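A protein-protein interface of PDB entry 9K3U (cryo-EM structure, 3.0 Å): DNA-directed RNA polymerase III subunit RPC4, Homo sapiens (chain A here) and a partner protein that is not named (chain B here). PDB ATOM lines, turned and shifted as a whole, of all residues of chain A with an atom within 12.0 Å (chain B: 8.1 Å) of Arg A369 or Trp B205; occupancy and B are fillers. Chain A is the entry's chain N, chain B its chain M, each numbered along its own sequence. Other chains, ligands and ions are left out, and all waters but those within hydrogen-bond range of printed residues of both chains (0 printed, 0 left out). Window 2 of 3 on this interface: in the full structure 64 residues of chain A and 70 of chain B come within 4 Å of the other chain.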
ATOM      1  N   VAL A 363     -14.055  13.497 -20.449  1.00  0.00           N
ATOM      2  CA  VAL A 363     -13.071  13.164 -21.473  1.00  0.00           C
ATOM      3  C   VAL A 363     -12.868  14.417 -22.316  1.00  0.00           C
ATOM      4  O   VAL A 363     -13.606  14.665 -23.274  1.00  0.00           O
ATOM      5  CB  VAL A 363     -13.518  11.969 -22.322  1.00  0.00           C
ATOM      6  CG1 VAL A 363     -12.516  11.702 -23.436  1.00  0.00           C
ATOM      7  CG2 VAL A 363     -13.693  10.732 -21.449  1.00  0.00           C
ATOM      8  N   GLY A 364     -11.862  15.211 -21.958  1.00  0.00           N
ATOM      9  CA  GLY A 364     -11.586  16.445 -22.666  1.00  0.00           C
ATOM     10  C   GLY A 364     -10.514  16.278 -23.723  1.00  0.00           C
ATOM     11  O   GLY A 364      -9.372  15.933 -23.412  1.00  0.00           O
ATOM     12  N   LEU A 365     -10.880  16.512 -24.985  1.00  0.00           N
ATOM     13  CA  LEU A 365      -9.945  16.397 -26.102  1.00  0.00           C
ATOM     14  C   LEU A 365      -9.321  17.767 -26.348  1.00  0.00           C
ATOM     15  O   LEU A 365      -9.640  18.476 -27.304  1.00  0.00           O
ATOM     16  CB  LEU A 365     -10.650  15.862 -27.343  1.00  0.00           C
ATOM     17  CG  LEU A 365     -11.091  14.396 -27.305  1.00  0.00           C
ATOM     18  CD1 LEU A 365     -12.215  14.177 -26.302  1.00  0.00           C
ATOM     19  CD2 LEU A 365     -11.512  13.931 -28.692  1.00  0.00           C
ATOM     20  N   GLY A 366      -8.409  18.143 -25.449  1.00  0.00           N
ATOM     21  CA  GLY A 366      -7.739  19.427 -25.587  1.00  0.00           C
ATOM     22  C   GLY A 366      -6.974  19.546 -26.890  1.00  0.00           C
ATOM     23  O   GLY A 366      -6.922  20.619 -27.495  1.00  0.00           O
ATOM     24  N   ASP A 367      -6.372  18.446 -27.339  1.00  0.00           N
ATOM     25  CA  ASP A 367      -5.645  18.399 -28.597  1.00  0.00           C
ATOM     26  C   ASP A 367      -6.289  17.371 -29.517  1.00  0.00           C
ATOM     27  O   ASP A 367      -6.898  16.398 -29.059  1.00  0.00           O
ATOM     28  CB  ASP A 367      -4.169  18.049 -28.373  1.00  0.00           C
ATOM     29  CG  ASP A 367      -3.347  18.129 -29.645  1.00  0.00           C
ATOM     30  OD1 ASP A 367      -3.903  18.532 -30.690  1.00  0.00           O
ATOM     31  OD2 ASP A 367      -2.145  17.792 -29.602  1.00  0.00           O
ATOM     32  N   SER A 368      -6.147  17.594 -30.825  1.00  0.00           N
ATOM     33  CA  SER A 368      -6.714  16.683 -31.810  1.00  0.00           C
ATOM     34  C   SER A 368      -6.012  15.332 -31.839  1.00  0.00           C
ATOM     35  O   SER A 368      -6.500  14.418 -32.511  1.00  0.00           O
ATOM     36  CB  SER A 368      -6.660  17.317 -33.200  1.00  0.00           C
ATOM     37  OG  SER A 368      -7.212  16.453 -34.178  1.00  0.00           O
ATOM     38  N   ARG A 369      -4.890  15.185 -31.134  1.00  0.00           N
ATOM     39  CA  ARG A 369      -4.138  13.937 -31.109  1.00  0.00           C
ATOM     40  C   ARG A 369      -4.122  13.266 -29.747  1.00  0.00           C
ATOM     41  O   ARG A 369      -4.023  12.039 -29.680  1.00  0.00           O
ATOM     42  CB  ARG A 369      -2.688  14.187 -31.555  1.00  0.00           C
ATOM     43  CG  ARG A 369      -1.811  12.940 -31.639  1.00  0.00           C
ATOM     44  CD  ARG A 369      -2.280  11.973 -32.718  1.00  0.00           C
ATOM     45  NE  ARG A 369      -3.416  11.164 -32.287  1.00  0.00           N
ATOM     46  CZ  ARG A 369      -4.011  10.245 -33.040  1.00  0.00           C
ATOM     47  NH1 ARG A 369      -3.583  10.009 -34.275  1.00  0.00           N
ATOM     48  NH2 ARG A 369      -5.040   9.559 -32.561  1.00  0.00           N
ATOM     49  N   THR A 370      -4.217  14.032 -28.660  1.00  0.00           N
ATOM     50  CA  THR A 370      -4.184  13.489 -27.308  1.00  0.00           C
ATOM     51  C   THR A 370      -5.168  14.252 -26.436  1.00  0.00           C
ATOM     52  O   THR A 370      -5.268  15.481 -26.534  1.00  0.00           O
ATOM     53  CB  THR A 370      -2.773  13.575 -26.711  1.00  0.00           C
ATOM     54  OG1 THR A 370      -1.850  12.872 -27.551  1.00  0.00           O
ATOM     55  CG2 THR A 370      -2.746  12.967 -25.313  1.00  0.00           C
ATOM     56  N   GLY A 371      -5.893  13.519 -25.586  1.00  0.00           N
ATOM     57  CA  GLY A 371      -6.835  14.107 -24.661  1.00  0.00           C
ATOM     58  C   GLY A 371      -6.566  13.635 -23.240  1.00  0.00           C
ATOM     59  O   GLY A 371      -5.583  12.939 -22.962  1.00  0.00           O
ATOM     60  N   GLU A 372      -7.460  14.028 -22.334  1.00  0.00           N
ATOM     61  CA  GLU A 372      -7.344  13.697 -20.921  1.00  0.00           C
ATOM     62  C   GLU A 372      -8.682  13.195 -20.395  1.00  0.00           C
ATOM     63  O   GLU A 372      -9.710  13.859 -20.560  1.00  0.00           O
ATOM     64  CB  GLU A 372      -6.882  14.912 -20.110  1.00  0.00           C
ATOM     65  CG  GLU A 372      -5.519  15.443 -20.524  1.00  0.00           C
ATOM     66  CD  GLU A 372      -5.085  16.637 -19.699  1.00  0.00           C
ATOM     67  OE1 GLU A 372      -5.851  17.056 -18.805  1.00  0.00           O
ATOM     68  OE2 GLU A 372      -3.976  17.160 -19.943  1.00  0.00           O
ATOM     69  N   MET A 373      -8.660  12.027 -19.754  1.00  0.00           N
ATOM     70  CA  MET A 373      -9.828  11.459 -19.092  1.00  0.00           C
ATOM     71  C   MET A 373      -9.674  11.670 -17.593  1.00  0.00           C
ATOM     72  O   MET A 373      -8.747  11.129 -16.980  1.00  0.00           O
ATOM     73  CB  MET A 373      -9.976   9.973 -19.415  1.00  0.00           C
ATOM     74  CG  MET A 373     -10.017   9.660 -20.903  1.00  0.00           C
ATOM     75  SD  MET A 373     -10.448   7.941 -21.249  1.00  0.00           S
ATOM     76  CE  MET A 373      -9.137   7.073 -20.389  1.00  0.00           C
ATOM     77  N   ALA B  47      -6.954   4.164 -23.752  1.00  0.00           N
ATOM     78  CA  ALA B  47      -8.363   4.076 -24.117  1.00  0.00           C
ATOM     79  C   ALA B  47      -8.535   4.552 -25.550  1.00  0.00           C
ATOM     80  O   ALA B  47      -8.105   5.656 -25.893  1.00  0.00           O
ATOM     81  CB  ALA B  47      -9.233   4.909 -23.170  1.00  0.00           C
ATOM     82  N   LYS B  48      -9.157   3.722 -26.382  1.00  0.00           N
ATOM     83  CA  LYS B  48      -9.456   4.086 -27.760  1.00  0.00           C
ATOM     84  C   LYS B  48     -10.863   4.664 -27.842  1.00  0.00           C
ATOM     85  O   LYS B  48     -11.807   4.107 -27.274  1.00  0.00           O
ATOM     86  CB  LYS B  48      -9.330   2.870 -28.678  1.00  0.00           C
ATOM     87  CG  LYS B  48      -7.955   2.218 -28.653  1.00  0.00           C
ATOM     88  CD  LYS B  48      -7.920   0.936 -29.471  1.00  0.00           C
ATOM     89  CE  LYS B  48      -8.129   1.203 -30.955  1.00  0.00           C
ATOM     90  NZ  LYS B  48      -8.019  -0.039 -31.766  1.00  0.00           N
ATOM     91  N   ILE B  49     -10.999   5.785 -28.552  1.00  0.00           N
ATOM     92  CA  ILE B  49     -12.265   6.504 -28.636  1.00  0.00           C
ATOM     93  C   ILE B  49     -12.406   7.085 -30.038  1.00  0.00           C
ATOM     94  O   ILE B  49     -11.481   7.042 -30.849  1.00  0.00           O
ATOM     95  CB  ILE B  49     -12.355   7.617 -27.563  1.00  0.00           C
ATOM     96  CG1 ILE B  49     -13.812   8.006 -27.293  1.00  0.00           C
ATOM     97  CG2 ILE B  49     -11.555   8.840 -27.994  1.00  0.00           C
ATOM     98  CD1 ILE B  49     -13.991   8.867 -26.063  1.00  0.00           C
ATOM     99  N   LYS B  50     -13.594   7.617 -30.324  1.00  0.00           N
ATOM    100  CA  LYS B  50     -13.862   8.323 -31.566  1.00  0.00           C
ATOM    101  C   LYS B  50     -14.723   9.546 -31.281  1.00  0.00           C
ATOM    102  O   LYS B  50     -15.632   9.483 -30.445  1.00  0.00           O
ATOM    103  CB  LYS B  50     -14.579   7.417 -32.579  1.00  0.00           C
ATOM    104  CG  LYS B  50     -13.775   6.206 -33.013  1.00  0.00           C
ATOM    105  CD  LYS B  50     -14.519   5.406 -34.069  1.00  0.00           C
ATOM    106  CE  LYS B  50     -13.730   4.180 -34.496  1.00  0.00           C
ATOM    107  NZ  LYS B  50     -14.445   3.390 -35.538  1.00  0.00           N
ATOM    108  N   PRO B  51     -14.469  10.673 -31.954  1.00  0.00           N
ATOM    109  CA  PRO B  51     -15.336  11.848 -31.734  1.00  0.00           C
ATOM    110  C   PRO B  51     -16.773  11.603 -32.161  1.00  0.00           C
ATOM    111  O   PRO B  51     -17.701  11.807 -31.367  1.00  0.00           O
ATOM    112  CB  PRO B  51     -14.656  12.940 -32.569  1.00  0.00           C
ATOM    113  CG  PRO B  51     -13.897  12.205 -33.618  1.00  0.00           C
ATOM    114  CD  PRO B  51     -13.436  10.931 -32.974  1.00  0.00           C
ATOM    115  N   GLN B  53     -19.823   8.989 -33.442  1.00  0.00           N
ATOM    116  CA  GLN B  53     -20.211   7.612 -33.134  1.00  0.00           C
ATOM    117  C   GLN B  53     -19.414   7.100 -31.933  1.00  0.00           C
ATOM    118  O   GLN B  53     -18.644   6.140 -32.018  1.00  0.00           O
ATOM    119  CB  GLN B  53     -20.023   6.710 -34.358  1.00  0.00           C
ATOM    120  CG  GLN B  53     -20.802   7.161 -35.582  1.00  0.00           C
ATOM    121  CD  GLN B  53     -20.501   6.323 -36.809  1.00  0.00           C
ATOM    122  OE1 GLN B  53     -19.651   5.434 -36.773  1.00  0.00           O
ATOM    123  NE2 GLN B  53     -21.200   6.603 -37.902  1.00  0.00           N
ATOM    124  N   GLN B  54     -19.616   7.772 -30.802  1.00  0.00           N
ATOM    125  CA  GLN B  54     -18.838   7.503 -29.600  1.00  0.00           C
ATOM    126  C   GLN B  54     -18.902   6.028 -29.226  1.00  0.00           C
ATOM    127  O   GLN B  54     -19.982   5.488 -28.965  1.00  0.00           O
ATOM    128  CB  GLN B  54     -19.344   8.370 -28.448  1.00  0.00           C
ATOM    129  CG  GLN B  54     -20.837   8.244 -28.177  1.00  0.00           C
ATOM    130  CD  GLN B  54     -21.309   9.158 -27.065  1.00  0.00           C
ATOM    131  OE1 GLN B  54     -20.504   9.810 -26.400  1.00  0.00           O
ATOM    132  NE2 GLN B  54     -22.619   9.210 -26.857  1.00  0.00           N
ATOM    133  N   LYS B  55     -17.740   5.379 -29.211  1.00  0.00           N
ATOM    134  CA  LYS B  55     -17.628   3.995 -28.751  1.00  0.00           C
ATOM    135  C   LYS B  55     -16.221   3.831 -28.182  1.00  0.00           C
ATOM    136  O   LYS B  55     -15.272   3.583 -28.933  1.00  0.00           O
ATOM    137  CB  LYS B  55     -17.899   3.010 -29.881  1.00  0.00           C
ATOM    138  CG  LYS B  55     -17.909   1.554 -29.440  1.00  0.00           C
ATOM    139  CD  LYS B  55     -18.376   0.629 -30.559  1.00  0.00           C
ATOM    140  CE  LYS B  55     -17.378   0.569 -31.706  1.00  0.00           C
ATOM    141  NZ  LYS B  55     -16.057   0.032 -31.278  1.00  0.00           N
ATOM    142  N   VAL B  56     -16.096   3.971 -26.868  1.00  0.00           N
ATOM    143  CA  VAL B  56     -14.802   3.947 -26.198  1.00  0.00           C
ATOM    144  C   VAL B  56     -14.446   2.513 -25.841  1.00  0.00           C
ATOM    145  O   VAL B  56     -15.312   1.718 -25.455  1.00  0.00           O
ATOM    146  CB  VAL B  56     -14.812   4.849 -24.948  1.00  0.00           C
ATOM    147  CG1 VAL B  56     -15.812   4.338 -23.915  1.00  0.00           C
ATOM    148  CG2 VAL B  56     -13.416   4.947 -24.348  1.00  0.00           C
ATOM    149  N   GLU B  57     -13.164   2.177 -25.971  1.00  0.00           N
ATOM    150  CA  GLU B  57     -12.641   0.861 -25.620  1.00  0.00           C
ATOM    151  C   GLU B  57     -11.470   1.061 -24.666  1.00  0.00           C
ATOM    152  O   GLU B  57     -10.438   1.622 -25.053  1.00  0.00           O
ATOM    153  CB  GLU B  57     -12.212   0.089 -26.866  1.00  0.00           C
ATOM    154  CG  GLU B  57     -11.691  -1.312 -26.581  1.00  0.00           C
ATOM    155  CD  GLU B  57     -11.308  -2.059 -27.844  1.00  0.00           C
ATOM    156  OE1 GLU B  57     -11.456  -1.486 -28.944  1.00  0.00           O
ATOM    157  OE2 GLU B  57     -10.859  -3.220 -27.735  1.00  0.00           O
ATOM    158  N   LEU B  58     -11.630   0.605 -23.427  1.00  0.00           N
ATOM    159  CA  LEU B  58     -10.610   0.778 -22.404  1.00  0.00           C
ATOM    160  C   LEU B  58      -9.648  -0.404 -22.405  1.00  0.00           C
ATOM    161  O   LEU B  58     -10.064  -1.559 -22.521  1.00  0.00           O
ATOM    162  CB  LEU B  58     -11.250   0.923 -21.023  1.00  0.00           C
ATOM    163  CG  LEU B  58     -12.236   2.083 -20.855  1.00  0.00           C
ATOM    164  CD1 LEU B  58     -12.788   2.107 -19.437  1.00  0.00           C
ATOM    165  CD2 LEU B  58     -11.580   3.409 -21.198  1.00  0.00           C
ATOM    166  N   CYS B 103     -15.386  -2.935 -23.685  1.00  0.00           N
ATOM    167  CA  CYS B 103     -16.015  -2.279 -24.819  1.00  0.00           C
ATOM    168  C   CYS B 103     -17.233  -1.491 -24.354  1.00  0.00           C
ATOM    169  O   CYS B 103     -17.906  -1.864 -23.388  1.00  0.00           O
ATOM    170  CB  CYS B 103     -16.434  -3.298 -25.885  1.00  0.00           C
ATOM    171  SG  CYS B 103     -17.286  -2.580 -27.309  1.00  0.00           S
ATOM    172  N   SER B 104     -17.511  -0.400 -25.059  1.00  0.00           N
ATOM    173  CA  SER B 104     -18.590   0.512 -24.713  1.00  0.00           C
ATOM    174  C   SER B 104     -19.770   0.316 -25.656  1.00  0.00           C
ATOM    175  O   SER B 104     -19.594   0.172 -26.869  1.00  0.00           O
ATOM    176  CB  SER B 104     -18.116   1.967 -24.778  1.00  0.00           C
ATOM    177  OG  SER B 104     -17.636   2.288 -26.072  1.00  0.00           O
ATOM    178  N   HIS B 200     -18.451   2.216 -39.430  1.00  0.00           N
ATOM    179  CA  HIS B 200     -17.946   2.602 -38.116  1.00  0.00           C
ATOM    180  C   HIS B 200     -16.428   2.487 -38.055  1.00  0.00           C
ATOM    181  O   HIS B 200     -15.761   3.338 -37.454  1.00  0.00           O
ATOM    182  CB  HIS B 200     -18.589   1.739 -37.029  1.00  0.00           C
ATOM    183  CG  HIS B 200     -20.014   2.093 -36.737  1.00  0.00           C
ATOM    184  ND1 HIS B 200     -20.380   3.287 -36.155  1.00  0.00           N
ATOM    185  CD2 HIS B 200     -21.163   1.404 -36.937  1.00  0.00           C
ATOM    186  CE1 HIS B 200     -21.694   3.322 -36.015  1.00  0.00           C
ATOM    187  NE2 HIS B 200     -22.193   2.193 -36.482  1.00  0.00           N
ATOM    188  N   ALA B 201     -15.865   1.445 -38.669  1.00  0.00           N
ATOM    189  CA  ALA B 201     -14.419   1.263 -38.652  1.00  0.00           C
ATOM    190  C   ALA B 201     -13.694   2.288 -39.511  1.00  0.00           C
ATOM    191  O   ALA B 201     -12.533   2.605 -39.228  1.00  0.00           O
ATOM    192  CB  ALA B 201     -14.061  -0.148 -39.118  1.00  0.00           C
ATOM    193  N   GLU B 202     -14.344   2.807 -40.557  1.00  0.00           N
ATOM    194  CA  GLU B 202     -13.698   3.800 -41.410  1.00  0.00           C
ATOM    195  C   GLU B 202     -13.199   4.996 -40.607  1.00  0.00           C
ATOM    196  O   GLU B 202     -12.169   5.586 -40.952  1.00  0.00           O
ATOM    197  CB  GLU B 202     -14.663   4.269 -42.499  1.00  0.00           C
ATOM    198  CG  GLU B 202     -14.777   3.318 -43.680  1.00  0.00           C
ATOM    199  CD  GLU B 202     -15.804   3.773 -44.698  1.00  0.00           C
ATOM    200  OE1 GLU B 202     -16.427   4.833 -44.482  1.00  0.00           O
ATOM    201  OE2 GLU B 202     -15.987   3.071 -45.714  1.00  0.00           O
ATOM    202  N   GLU B 203     -13.903   5.365 -39.546  1.00  0.00           N
ATOM    203  CA  GLU B 203     -13.484   6.503 -38.739  1.00  0.00           C
ATOM    204  C   GLU B 203     -12.224   6.143 -37.958  1.00  0.00           C
ATOM    205  O   GLU B 203     -12.165   5.069 -37.348  1.00  0.00           O
ATOM    206  CB  GLU B 203     -14.603   6.915 -37.781  1.00  0.00           C
ATOM    207  CG  GLU B 203     -14.281   8.144 -36.946  1.00  0.00           C
ATOM    208  CD  GLU B 203     -15.438   8.562 -36.058  1.00  0.00           C
ATOM    209  OE1 GLU B 203     -16.497   7.903 -36.111  1.00  0.00           O
ATOM    210  OE2 GLU B 203     -15.287   9.549 -35.309  1.00  0.00           O
ATOM    211  N   PRO B 204     -11.203   6.999 -37.947  1.00  0.00           N
ATOM    212  CA  PRO B 204      -9.975   6.664 -37.221  1.00  0.00           C
ATOM    213  C   PRO B 204     -10.173   6.726 -35.715  1.00  0.00           C
ATOM    214  O   PRO B 204     -11.048   7.427 -35.198  1.00  0.00           O
ATOM    215  CB  PRO B 204      -8.980   7.729 -37.696  1.00  0.00           C
ATOM    216  CG  PRO B 204      -9.831   8.891 -38.059  1.00  0.00           C
ATOM    217  CD  PRO B 204     -11.113   8.318 -38.599  1.00  0.00           C
ATOM    218  N   TRP B 205      -9.338   5.972 -35.009  1.00  0.00           N
ATOM    219  CA  TRP B 205      -9.373   5.930 -33.555  1.00  0.00           C
ATOM    220  C   TRP B 205      -8.508   7.039 -32.967  1.00  0.00           C
ATOM    221  O   TRP B 205      -7.669   7.631 -33.650  1.00  0.00           O
ATOM    222  CB  TRP B 205      -8.885   4.573 -33.041  1.00  0.00           C
ATOM    223  CG  TRP B 205      -9.774   3.424 -33.409  1.00  0.00           C
ATOM    224  CD1 TRP B 205      -9.664   2.620 -34.506  1.00  0.00           C
ATOM    225  CD2 TRP B 205     -10.907   2.951 -32.676  1.00  0.00           C
ATOM    226  NE1 TRP B 205     -10.659   1.673 -34.501  1.00  0.00           N
ATOM    227  CE2 TRP B 205     -11.437   1.856 -33.388  1.00  0.00           C
ATOM    228  CE3 TRP B 205     -11.529   3.345 -31.487  1.00  0.00           C
ATOM    229  CZ2 TRP B 205     -12.557   1.150 -32.950  1.00  0.00           C
ATOM    230  CZ3 TRP B 205     -12.639   2.645 -31.054  1.00  0.00           C
ATOM    231  CH2 TRP B 205     -13.142   1.560 -31.783  1.00  0.00           C
ATOM    232  N   VAL B 206      -8.727   7.315 -31.683  1.00  0.00           N
ATOM    233  CA  VAL B 206      -7.941   8.284 -30.933  1.00  0.00           C
ATOM    234  C   VAL B 206      -7.565   7.647 -29.603  1.00  0.00           C
ATOM    235  O   VAL B 206      -8.434   7.132 -28.890  1.00  0.00           O
ATOM    236  CB  VAL B 206      -8.714   9.599 -30.705  1.00  0.00           C
ATOM    237  CG1 VAL B 206      -7.830  10.617 -29.986  1.00  0.00           C
ATOM    238  CG2 VAL B 206      -9.227  10.147 -32.033  1.00  0.00           C
ATOM    239  N   HIS B 207      -6.275   7.676 -29.279  1.00  0.00           N
ATOM    240  CA  HIS B 207      -5.773   7.095 -28.043  1.00  0.00           C
ATOM    241  C   HIS B 207      -5.704   8.156 -26.953  1.00  0.00           C
ATOM    242  O   HIS B 207      -5.225   9.270 -27.180  1.00  0.00           O
ATOM    243  CB  HIS B 207      -4.388   6.480 -28.262  1.00  0.00           C
ATOM    244  CG  HIS B 207      -4.365   5.397 -29.295  1.00  0.00           C
ATOM    245  ND1 HIS B 207      -4.667   5.627 -30.621  1.00  0.00           N
ATOM    246  CD2 HIS B 207      -4.078   4.077 -29.199  1.00  0.00           C
ATOM    247  CE1 HIS B 207      -4.564   4.494 -31.296  1.00  0.00           C
ATOM    248  NE2 HIS B 207      -4.210   3.539 -30.455  1.00  0.00           N
ATOM    249  N   LEU B 208      -6.180   7.796 -25.763  1.00  0.00           N
ATOM    250  CA  LEU B 208      -6.206   8.693 -24.619  1.00  0.00           C
ATOM    251  C   LEU B 208      -5.607   7.989 -23.412  1.00  0.00           C
ATOM    252  O   LEU B 208      -5.750   6.774 -23.243  1.00  0.00           O
ATOM    253  CB  LEU B 208      -7.637   9.146 -24.290  1.00  0.00           C
ATOM    254  CG  LEU B 208      -8.459   9.728 -25.440  1.00  0.00           C
ATOM    255  CD1 LEU B 208      -9.870  10.037 -24.968  1.00  0.00           C
ATOM    256  CD2 LEU B 208      -7.803  10.973 -26.006  1.00  0.00           C
ATOM    257  N   HIS B 209      -4.937   8.769 -22.570  1.00  0.00           N
ATOM    258  CA  HIS B 209      -4.377   8.269 -21.326  1.00  0.00           C
ATOM    259  C   HIS B 209      -5.431   8.309 -20.224  1.00  0.00           C
ATOM    260  O   HIS B 209      -6.431   9.026 -20.310  1.00  0.00           O
ATOM    261  CB  HIS B 209      -3.153   9.090 -20.915  1.00  0.00           C
ATOM    262  CG  HIS B 209      -2.079   9.133 -21.956  1.00  0.00           C
ATOM    263  ND1 HIS B 209      -2.219   9.822 -23.142  1.00  0.00           N
ATOM    264  CD2 HIS B 209      -0.847   8.571 -21.992  1.00  0.00           C
ATOM    265  CE1 HIS B 209      -1.120   9.685 -23.861  1.00  0.00           C
ATOM    266  NE2 HIS B 209      -0.272   8.930 -23.186  1.00  0.00           N
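The backbone carbonyl oxygen (O) of Trp B205 sits at hydrogen-bond distance from the guanidinium group (NH2) of Arg A369, 3.4 Å away.
The backbone carbonyl oxygen of Ile B49 is in hydrogen-bond range of the backbone NH of Val B206, at 2.9 Å. The backbone carbonyl oxygen (O) of Ala B47 sits at hydrogen-bond distance from the backbone NH (N) of Leu B208, 2.9 Å away.
CD1 of Leu B208 touches CG1 of Val A363, at 3.5 Å. NH2 of Arg A369 touches CA of Val B206, at 3.6 Å. His B207 touches Arg A369 (O to O, 3.9 Å). ND1 of His B209 touches CG2 of Thr A370, 3.9 Å away. Gly A371 touches Leu B208. CE of Met A373 touches CB of Ala B47, 3.5 Å away. O of His B209 touches CE of Met A373, at 3.3 Å.
Gly A364 touches none of the printed residues of chain B. Of chain B, only Trp B205 (3.4 Å), Val B206 (3.6 Å) and His B207 (3.9 Å) come within 4 Å of Arg A369. Of the printed residues of chain B, Gly A371 touches Leu B208 (3.2 Å). Printed residues of chain B within 4 Å of Met A373: Ala B47 and His B209. Of the printed residues of chain A, Ala B47 touches Met A373 (3.5 Å). Lys B48 touches none of the printed residues of chain A. Lys B55 touches none of the printed residues of chain A. Val B56 touches none of the printed residues of chain A. No residue of chain A comes within 4 Å of Glu B203. Trp B205 touches one residue of chain A. Of chain A, only Arg A369 comes within 4 Å of Val B206. His B207 touches just one residue of chain A: Arg A369. Printed residues of chain A within 4 Å of Leu B208: Val A363 (3.5 Å) and Gly A371 (3.2 Å). Printed residues of chain A within 4 Å of His B209: Thr A370 (3.9 Å) and Met A373 (3.3 Å). The nearest residue of chain B that does not touch Arg A369 is Leu B208 (5.4 Å). The nearest residue of chain A that does not touch Trp B205 is Ser A368 (7.0 Å).
Of the 23 printed residues of chain B, 6 touch a printed residue of chain A. Hydrophobic or aromatic side chains of chain B that line the printed part of chain A: Ala B47, Val B206, Leu B208 and His B209. Among the printed residues, 8 pairs touch across the chains. Among the printed residues, no Asp or Glu carboxylate lies within 4 Å of a Lys or Arg side-chain nitrogen of the other chain.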
